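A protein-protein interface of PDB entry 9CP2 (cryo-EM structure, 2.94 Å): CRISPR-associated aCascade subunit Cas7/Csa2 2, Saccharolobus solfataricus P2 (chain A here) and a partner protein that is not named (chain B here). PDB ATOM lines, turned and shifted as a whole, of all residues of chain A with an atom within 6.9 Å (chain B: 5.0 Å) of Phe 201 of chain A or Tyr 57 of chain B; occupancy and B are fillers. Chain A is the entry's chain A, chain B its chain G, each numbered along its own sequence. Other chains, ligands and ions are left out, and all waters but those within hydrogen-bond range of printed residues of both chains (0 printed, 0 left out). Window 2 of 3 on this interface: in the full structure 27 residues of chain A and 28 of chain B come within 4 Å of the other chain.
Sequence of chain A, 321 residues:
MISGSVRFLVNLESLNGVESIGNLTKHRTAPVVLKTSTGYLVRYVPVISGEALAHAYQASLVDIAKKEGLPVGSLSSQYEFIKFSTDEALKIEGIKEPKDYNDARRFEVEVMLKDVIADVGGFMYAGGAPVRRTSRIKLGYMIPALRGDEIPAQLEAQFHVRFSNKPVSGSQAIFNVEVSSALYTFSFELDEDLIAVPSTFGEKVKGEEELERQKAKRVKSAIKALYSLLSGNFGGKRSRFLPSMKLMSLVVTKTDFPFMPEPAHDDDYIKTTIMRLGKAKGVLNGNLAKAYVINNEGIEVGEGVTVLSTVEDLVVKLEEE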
ATOM      1  N   TYR A 101      -5.305 -13.560 -36.011  1.00  0.00           N
ATOM      2  CA  TYR A 101      -4.984 -14.168 -34.723  1.00  0.00           C
ATOM      3  C   TYR A 101      -4.968 -13.132 -33.607  1.00  0.00           C
ATOM      4  O   TYR A 101      -5.424 -13.409 -32.491  1.00  0.00           O
ATOM      5  CB  TYR A 101      -3.637 -14.885 -34.806  1.00  0.00           C
ATOM      6  CG  TYR A 101      -3.535 -15.866 -35.951  1.00  0.00           C
ATOM      7  CD1 TYR A 101      -4.130 -17.119 -35.874  1.00  0.00           C
ATOM      8  CD2 TYR A 101      -2.843 -15.539 -37.111  1.00  0.00           C
ATOM      9  CE1 TYR A 101      -4.038 -18.019 -36.918  1.00  0.00           C
ATOM     10  CE2 TYR A 101      -2.748 -16.433 -38.161  1.00  0.00           C
ATOM     11  CZ  TYR A 101      -3.346 -17.671 -38.060  1.00  0.00           C
ATOM     12  OH  TYR A 101      -3.252 -18.564 -39.102  1.00  0.00           O
ATOM     13  N   ASN A 102      -4.460 -11.931 -33.892  1.00  0.00           N
ATOM     14  CA  ASN A 102      -4.303 -10.921 -32.850  1.00  0.00           C
ATOM     15  C   ASN A 102      -5.645 -10.528 -32.248  1.00  0.00           C
ATOM     16  O   ASN A 102      -5.754 -10.324 -31.033  1.00  0.00           O
ATOM     17  CB  ASN A 102      -3.591  -9.694 -33.417  1.00  0.00           C
ATOM     18  CG  ASN A 102      -2.084  -9.816 -33.349  1.00  0.00           C
ATOM     19  OD1 ASN A 102      -1.452  -9.330 -32.412  1.00  0.00           O
ATOM     20  ND2 ASN A 102      -1.499 -10.468 -34.346  1.00  0.00           N
ATOM     21  N   ALA A 104      -8.123 -12.445 -31.969  1.00  0.00           N
ATOM     22  CA  ALA A 104      -8.808 -13.643 -31.491  1.00  0.00           C
ATOM     23  C   ALA A 104      -9.303 -13.471 -30.062  1.00  0.00           C
ATOM     24  O   ALA A 104     -10.493 -13.658 -29.779  1.00  0.00           O
ATOM     25  CB  ALA A 104      -7.878 -14.851 -31.598  1.00  0.00           C
ATOM     26  N   ARG A 105      -8.407 -13.069 -29.156  1.00  0.00           N
ATOM     27  CA  ARG A 105      -8.802 -12.831 -27.772  1.00  0.00           C
ATOM     28  C   ARG A 105     -10.015 -11.919 -27.706  1.00  0.00           C
ATOM     29  O   ARG A 105     -11.028 -12.255 -27.080  1.00  0.00           O
ATOM     30  CB  ARG A 105      -7.638 -12.223 -26.989  1.00  0.00           C
ATOM     31  CG  ARG A 105      -7.981 -11.890 -25.550  1.00  0.00           C
ATOM     32  CD  ARG A 105      -6.748 -11.823 -24.670  1.00  0.00           C
ATOM     33  NE  ARG A 105      -7.101 -11.909 -23.259  1.00  0.00           N
ATOM     34  CZ  ARG A 105      -6.253 -12.227 -22.292  1.00  0.00           C
ATOM     35  NH1 ARG A 105      -4.984 -12.496 -22.546  1.00  0.00           N
ATOM     36  NH2 ARG A 105      -6.691 -12.280 -21.037  1.00  0.00           N
ATOM     37  N   PRO A 130      -9.118 -20.074 -36.445  1.00  0.00           N
ATOM     38  CA  PRO A 130      -9.823 -20.862 -35.428  1.00  0.00           C
ATOM     39  C   PRO A 130      -9.568 -20.333 -34.026  1.00  0.00           C
ATOM     40  O   PRO A 130      -8.462 -19.904 -33.692  1.00  0.00           O
ATOM     41  CB  PRO A 130      -9.248 -22.270 -35.612  1.00  0.00           C
ATOM     42  CG  PRO A 130      -7.909 -22.048 -36.232  1.00  0.00           C
ATOM     43  CD  PRO A 130      -8.072 -20.854 -37.124  1.00  0.00           C
ATOM     44  N   PRO A 198     -10.305 -15.385 -19.699  1.00  0.00           N
ATOM     45  CA  PRO A 198      -9.953 -15.646 -21.099  1.00  0.00           C
ATOM     46  C   PRO A 198      -8.841 -16.679 -21.196  1.00  0.00           C
ATOM     47  O   PRO A 198      -8.008 -16.814 -20.299  1.00  0.00           O
ATOM     48  CB  PRO A 198      -9.493 -14.278 -21.611  1.00  0.00           C
ATOM     49  CG  PRO A 198     -10.153 -13.297 -20.708  1.00  0.00           C
ATOM     50  CD  PRO A 198     -10.217 -13.956 -19.363  1.00  0.00           C
ATOM     51  N   SER A 199      -8.836 -17.415 -22.304  1.00  0.00           N
ATOM     52  CA  SER A 199      -7.929 -18.539 -22.504  1.00  0.00           C
ATOM     53  C   SER A 199      -7.020 -18.314 -23.705  1.00  0.00           C
ATOM     54  O   SER A 199      -6.818 -19.206 -24.530  1.00  0.00           O
ATOM     55  CB  SER A 199      -8.712 -19.840 -22.660  1.00  0.00           C
ATOM     56  OG  SER A 199      -7.850 -20.963 -22.606  1.00  0.00           O
ATOM     57  N   THR A 200      -6.460 -17.113 -23.817  1.00  0.00           N
ATOM     58  CA  THR A 200      -5.530 -16.794 -24.891  1.00  0.00           C
ATOM     59  C   THR A 200      -4.589 -15.702 -24.407  1.00  0.00           C
ATOM     60  O   THR A 200      -5.004 -14.799 -23.678  1.00  0.00           O
ATOM     61  CB  THR A 200      -6.263 -16.337 -26.159  1.00  0.00           C
ATOM     62  OG1 THR A 200      -7.352 -17.225 -26.437  1.00  0.00           O
ATOM     63  CG2 THR A 200      -5.319 -16.322 -27.349  1.00  0.00           C
ATOM     64  N   PHE A 201      -3.324 -15.789 -24.811  1.00  0.00           N
ATOM     65  CA  PHE A 201      -2.360 -14.763 -24.442  1.00  0.00           C
ATOM     66  C   PHE A 201      -2.533 -13.513 -25.292  1.00  0.00           C
ATOM     67  O   PHE A 201      -2.750 -13.584 -26.505  1.00  0.00           O
ATOM     68  CB  PHE A 201      -0.931 -15.287 -24.572  1.00  0.00           C
ATOM     69  CG  PHE A 201      -0.448 -16.023 -23.361  1.00  0.00           C
ATOM     70  CD1 PHE A 201       0.043 -15.327 -22.269  1.00  0.00           C
ATOM     71  CD2 PHE A 201      -0.482 -17.404 -23.308  1.00  0.00           C
ATOM     72  CE1 PHE A 201       0.492 -15.994 -21.148  1.00  0.00           C
ATOM     73  CE2 PHE A 201      -0.032 -18.077 -22.189  1.00  0.00           C
ATOM     74  CZ  PHE A 201       0.455 -17.370 -21.107  1.00  0.00           C
ATOM     75  N   GLY A 202      -2.435 -12.365 -24.640  1.00  0.00           N
ATOM     76  CA  GLY A 202      -2.542 -11.091 -25.316  1.00  0.00           C
ATOM     77  C   GLY A 202      -2.780  -9.986 -24.312  1.00  0.00           C
ATOM     78  O   GLY A 202      -2.945 -10.221 -23.115  1.00  0.00           O
ATOM     79  N   GLU A 203      -2.794  -8.762 -24.832  1.00  0.00           N
ATOM     80  CA  GLU A 203      -3.074  -7.601 -24.005  1.00  0.00           C
ATOM     81  C   GLU A 203      -4.546  -7.571 -23.616  1.00  0.00           C
ATOM     82  O   GLU A 203      -5.411  -8.068 -24.343  1.00  0.00           O
ATOM     83  CB  GLU A 203      -2.703  -6.315 -24.742  1.00  0.00           C
ATOM     84  CG  GLU A 203      -1.410  -6.408 -25.533  1.00  0.00           C
ATOM     85  CD  GLU A 203      -1.011  -5.084 -26.151  1.00  0.00           C
ATOM     86  OE1 GLU A 203      -1.769  -4.102 -25.998  1.00  0.00           O
ATOM     87  OE2 GLU A 203       0.060  -5.024 -26.789  1.00  0.00           O
ATOM     88  N   VAL B  48      -4.196 -22.169 -20.153  1.00  0.00           N
ATOM     89  CA  VAL B  48      -3.996 -21.536 -21.449  1.00  0.00           C
ATOM     90  C   VAL B  48      -4.196 -22.576 -22.541  1.00  0.00           C
ATOM     91  O   VAL B  48      -3.825 -23.744 -22.379  1.00  0.00           O
ATOM     92  CB  VAL B  48      -2.605 -20.871 -21.562  1.00  0.00           C
ATOM     93  CG1 VAL B  48      -2.385 -19.919 -20.401  1.00  0.00           C
ATOM     94  CG2 VAL B  48      -1.503 -21.912 -21.612  1.00  0.00           C
ATOM     95  N   ASN B  50      -3.774 -21.354 -26.050  1.00  0.00           N
ATOM     96  CA  ASN B  50      -3.137 -20.807 -27.240  1.00  0.00           C
ATOM     97  C   ASN B  50      -1.979 -19.921 -26.813  1.00  0.00           C
ATOM     98  O   ASN B  50      -2.126 -19.103 -25.901  1.00  0.00           O
ATOM     99  CB  ASN B  50      -4.134 -20.010 -28.085  1.00  0.00           C
ATOM    100  CG  ASN B  50      -4.754 -20.839 -29.188  1.00  0.00           C
ATOM    101  OD1 ASN B  50      -4.085 -21.662 -29.809  1.00  0.00           O
ATOM    102  ND2 ASN B  50      -6.040 -20.626 -29.437  1.00  0.00           N
ATOM    103  N   ILE B  51      -0.831 -20.096 -27.465  1.00  0.00           N
ATOM    104  CA  ILE B  51       0.333 -19.250 -27.251  1.00  0.00           C
ATOM    105  C   ILE B  51       0.910 -18.886 -28.609  1.00  0.00           C
ATOM    106  O   ILE B  51       0.697 -19.574 -29.608  1.00  0.00           O
ATOM    107  CB  ILE B  51       1.411 -19.927 -26.377  1.00  0.00           C
ATOM    108  CG1 ILE B  51       1.840 -21.258 -26.990  1.00  0.00           C
ATOM    109  CG2 ILE B  51       0.901 -20.145 -24.967  1.00  0.00           C
ATOM    110  CD1 ILE B  51       3.100 -21.821 -26.373  1.00  0.00           C
ATOM    111  N   ASN B  52       1.657 -17.786 -28.635  1.00  0.00           N
ATOM    112  CA  ASN B  52       2.298 -17.319 -29.861  1.00  0.00           C
ATOM    113  C   ASN B  52       3.716 -17.872 -29.894  1.00  0.00           C
ATOM    114  O   ASN B  52       4.601 -17.389 -29.183  1.00  0.00           O
ATOM    115  CB  ASN B  52       2.286 -15.796 -29.932  1.00  0.00           C
ATOM    116  CG  ASN B  52       2.855 -15.270 -31.233  1.00  0.00           C
ATOM    117  OD1 ASN B  52       2.810 -15.946 -32.262  1.00  0.00           O
ATOM    118  ND2 ASN B  52       3.395 -14.059 -31.197  1.00  0.00           N
ATOM    119  N   LEU B  53       3.934 -18.893 -30.724  1.00  0.00           N
ATOM    120  CA  LEU B  53       5.264 -19.470 -30.868  1.00  0.00           C
ATOM    121  C   LEU B  53       6.235 -18.515 -31.547  1.00  0.00           C
ATOM    122  O   LEU B  53       7.449 -18.738 -31.489  1.00  0.00           O
ATOM    123  CB  LEU B  53       5.188 -20.776 -31.659  1.00  0.00           C
ATOM    124  CG  LEU B  53       4.177 -21.809 -31.164  1.00  0.00           C
ATOM    125  CD1 LEU B  53       4.152 -23.015 -32.088  1.00  0.00           C
ATOM    126  CD2 LEU B  53       4.498 -22.226 -29.742  1.00  0.00           C
ATOM    127  N   ASN B  55       5.420 -17.327 -34.890  1.00  0.00           N
ATOM    128  CA  ASN B  55       4.808 -17.210 -36.207  1.00  0.00           C
ATOM    129  C   ASN B  55       3.440 -17.864 -36.319  1.00  0.00           C
ATOM    130  O   ASN B  55       2.755 -17.622 -37.317  1.00  0.00           O
ATOM    131  CB  ASN B  55       5.731 -17.813 -37.276  1.00  0.00           C
ATOM    132  CG  ASN B  55       7.101 -17.166 -37.294  1.00  0.00           C
ATOM    133  OD1 ASN B  55       7.315 -16.155 -37.963  1.00  0.00           O
ATOM    134  ND2 ASN B  55       8.038 -17.747 -36.554  1.00  0.00           N
ATOM    135  N   VAL B  56       3.012 -18.671 -35.348  1.00  0.00           N
ATOM    136  CA  VAL B  56       1.742 -19.383 -35.443  1.00  0.00           C
ATOM    137  C   VAL B  56       1.342 -19.829 -34.045  1.00  0.00           C
ATOM    138  O   VAL B  56       2.195 -20.107 -33.199  1.00  0.00           O
ATOM    139  CB  VAL B  56       1.848 -20.577 -36.425  1.00  0.00           C
ATOM    140  CG1 VAL B  56       2.904 -21.566 -35.953  1.00  0.00           C
ATOM    141  CG2 VAL B  56       0.496 -21.255 -36.610  1.00  0.00           C
ATOM    142  N   TYR B  57       0.032 -19.887 -33.801  1.00  0.00           N
ATOM    143  CA  TYR B  57      -0.522 -20.325 -32.521  1.00  0.00           C
ATOM    144  C   TYR B  57      -0.648 -21.842 -32.561  1.00  0.00           C
ATOM    145  O   TYR B  57      -1.664 -22.388 -32.990  1.00  0.00           O
ATOM    146  CB  TYR B  57      -1.875 -19.669 -32.276  1.00  0.00           C
ATOM    147  CG  TYR B  57      -1.818 -18.269 -31.710  1.00  0.00           C
ATOM    148  CD1 TYR B  57      -1.696 -17.169 -32.548  1.00  0.00           C
ATOM    149  CD2 TYR B  57      -1.919 -18.044 -30.345  1.00  0.00           C
ATOM    150  CE1 TYR B  57      -1.652 -15.886 -32.041  1.00  0.00           C
ATOM    151  CE2 TYR B  57      -1.879 -16.763 -29.828  1.00  0.00           C
ATOM    152  CZ  TYR B  57      -1.745 -15.688 -30.680  1.00  0.00           C
ATOM    153  OH  TYR B  57      -1.704 -14.411 -30.169  1.00  0.00           O
ATOM    154  N   GLY B  58       0.390 -22.543 -32.113  1.00  0.00           N
ATOM    155  CA  GLY B  58       0.350 -23.989 -32.204  1.00  0.00           C
ATOM    156  C   GLY B  58      -0.287 -24.716 -31.036  1.00  0.00           C
ATOM    157  O   GLY B  58      -1.321 -25.365 -31.207  1.00  0.00           O
ATOM    158  N   SER B  59       0.301 -24.600 -29.843  1.00  0.00           N
ATOM    159  CA  SER B  59      -0.185 -25.276 -28.644  1.00  0.00           C
ATOM    160  C   SER B  59       0.674 -24.874 -27.452  1.00  0.00           C
ATOM    161  O   SER B  59       1.829 -24.470 -27.636  1.00  0.00           O
ATOM    162  CB  SER B  59      -0.166 -26.797 -28.817  1.00  0.00           C
ATOM    163  OG  SER B  59       1.145 -27.269 -29.057  1.00  0.00           O
ATOM    164  N   TRP B 199      -1.716 -26.298 -35.384  1.00  0.00           N
ATOM    165  CA  TRP B 199      -2.971 -26.501 -36.096  1.00  0.00           C
ATOM    166  C   TRP B 199      -2.767 -26.343 -37.597  1.00  0.00           C
ATOM    167  O   TRP B 199      -1.892 -25.606 -38.057  1.00  0.00           O
ATOM    168  CB  TRP B 199      -4.043 -25.514 -35.625  1.00  0.00           C
ATOM    169  CG  TRP B 199      -4.088 -25.261 -34.151  1.00  0.00           C
ATOM    170  CD1 TRP B 199      -4.099 -24.047 -33.536  1.00  0.00           C
ATOM    171  CD2 TRP B 199      -4.155 -26.239 -33.108  1.00  0.00           C
ATOM    172  NE1 TRP B 199      -4.157 -24.205 -32.175  1.00  0.00           N
ATOM    173  CE2 TRP B 199      -4.195 -25.543 -31.887  1.00  0.00           C
ATOM    174  CE3 TRP B 199      -4.182 -27.636 -33.088  1.00  0.00           C
ATOM    175  CZ2 TRP B 199      -4.255 -26.194 -30.660  1.00  0.00           C
ATOM    176  CZ3 TRP B 199      -4.242 -28.278 -31.871  1.00  0.00           C
ATOM    177  CH2 TRP B 199      -4.274 -27.559 -30.674  1.00  0.00           C
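The guanidinium group (NH1) of Arg 105 of chain A lies within hydrogen-bond range of the backbone carbonyl oxygen (O) of Thr 200 of chain A (2.6 Å).
The indole nitrogen (NE1) of Trp 199 of chain B lies within hydrogen-bond range of the side-chain amide oxygen (OD1) of Asn 50 of chain B (3.5 Å).
The indole nitrogen (NE1) of Trp 199 of chain B sits close to the backbone carbonyl oxygen (O) of Tyr 57 of chain B (3.2 Å).
Among the printed residues, pairs that only touch across the chains: Phe 201 of chain A with Val 48 of chain B (3.5 Å), Phe 201 of chain A with Ile 51 of chain B (3.5 Å), Phe 201 of chain A with Asn 50 of chain B (3.5 Å), Tyr 101 of chain A with Tyr 57 of chain B (3.5 Å), Phe 201 of chain A with Tyr 57 of chain B (3.9 Å), Thr 200 of chain A with Asn 50 of chain B (3.9 Å) and Ser 199 of chain A with Val 48 of chain B (3.99 Å).
Printed residues of chain B within 4 Å of Ser 199 of chain A: Val 48.
Printed residues of chain A within 4 Å of Ile 51 of chain B: Phe 201.
Of the printed residues of chain B, Thr 200 of chain A touches Asn 50.
Printed residues of chain A within 4 Å of Val 48 of chain B: Ser 199 and Phe 201.
Asn 102 of chain A touches none of the printed residues of chain B.
The nearest residue of chain A that does not touch Tyr 57 of chain B is Thr 200 of chain A (4.3 Å).
Of the 11 printed residues of chain B, 4 touch a printed residue of chain A.
Among the printed residues, 7 pairs touch across the chains.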
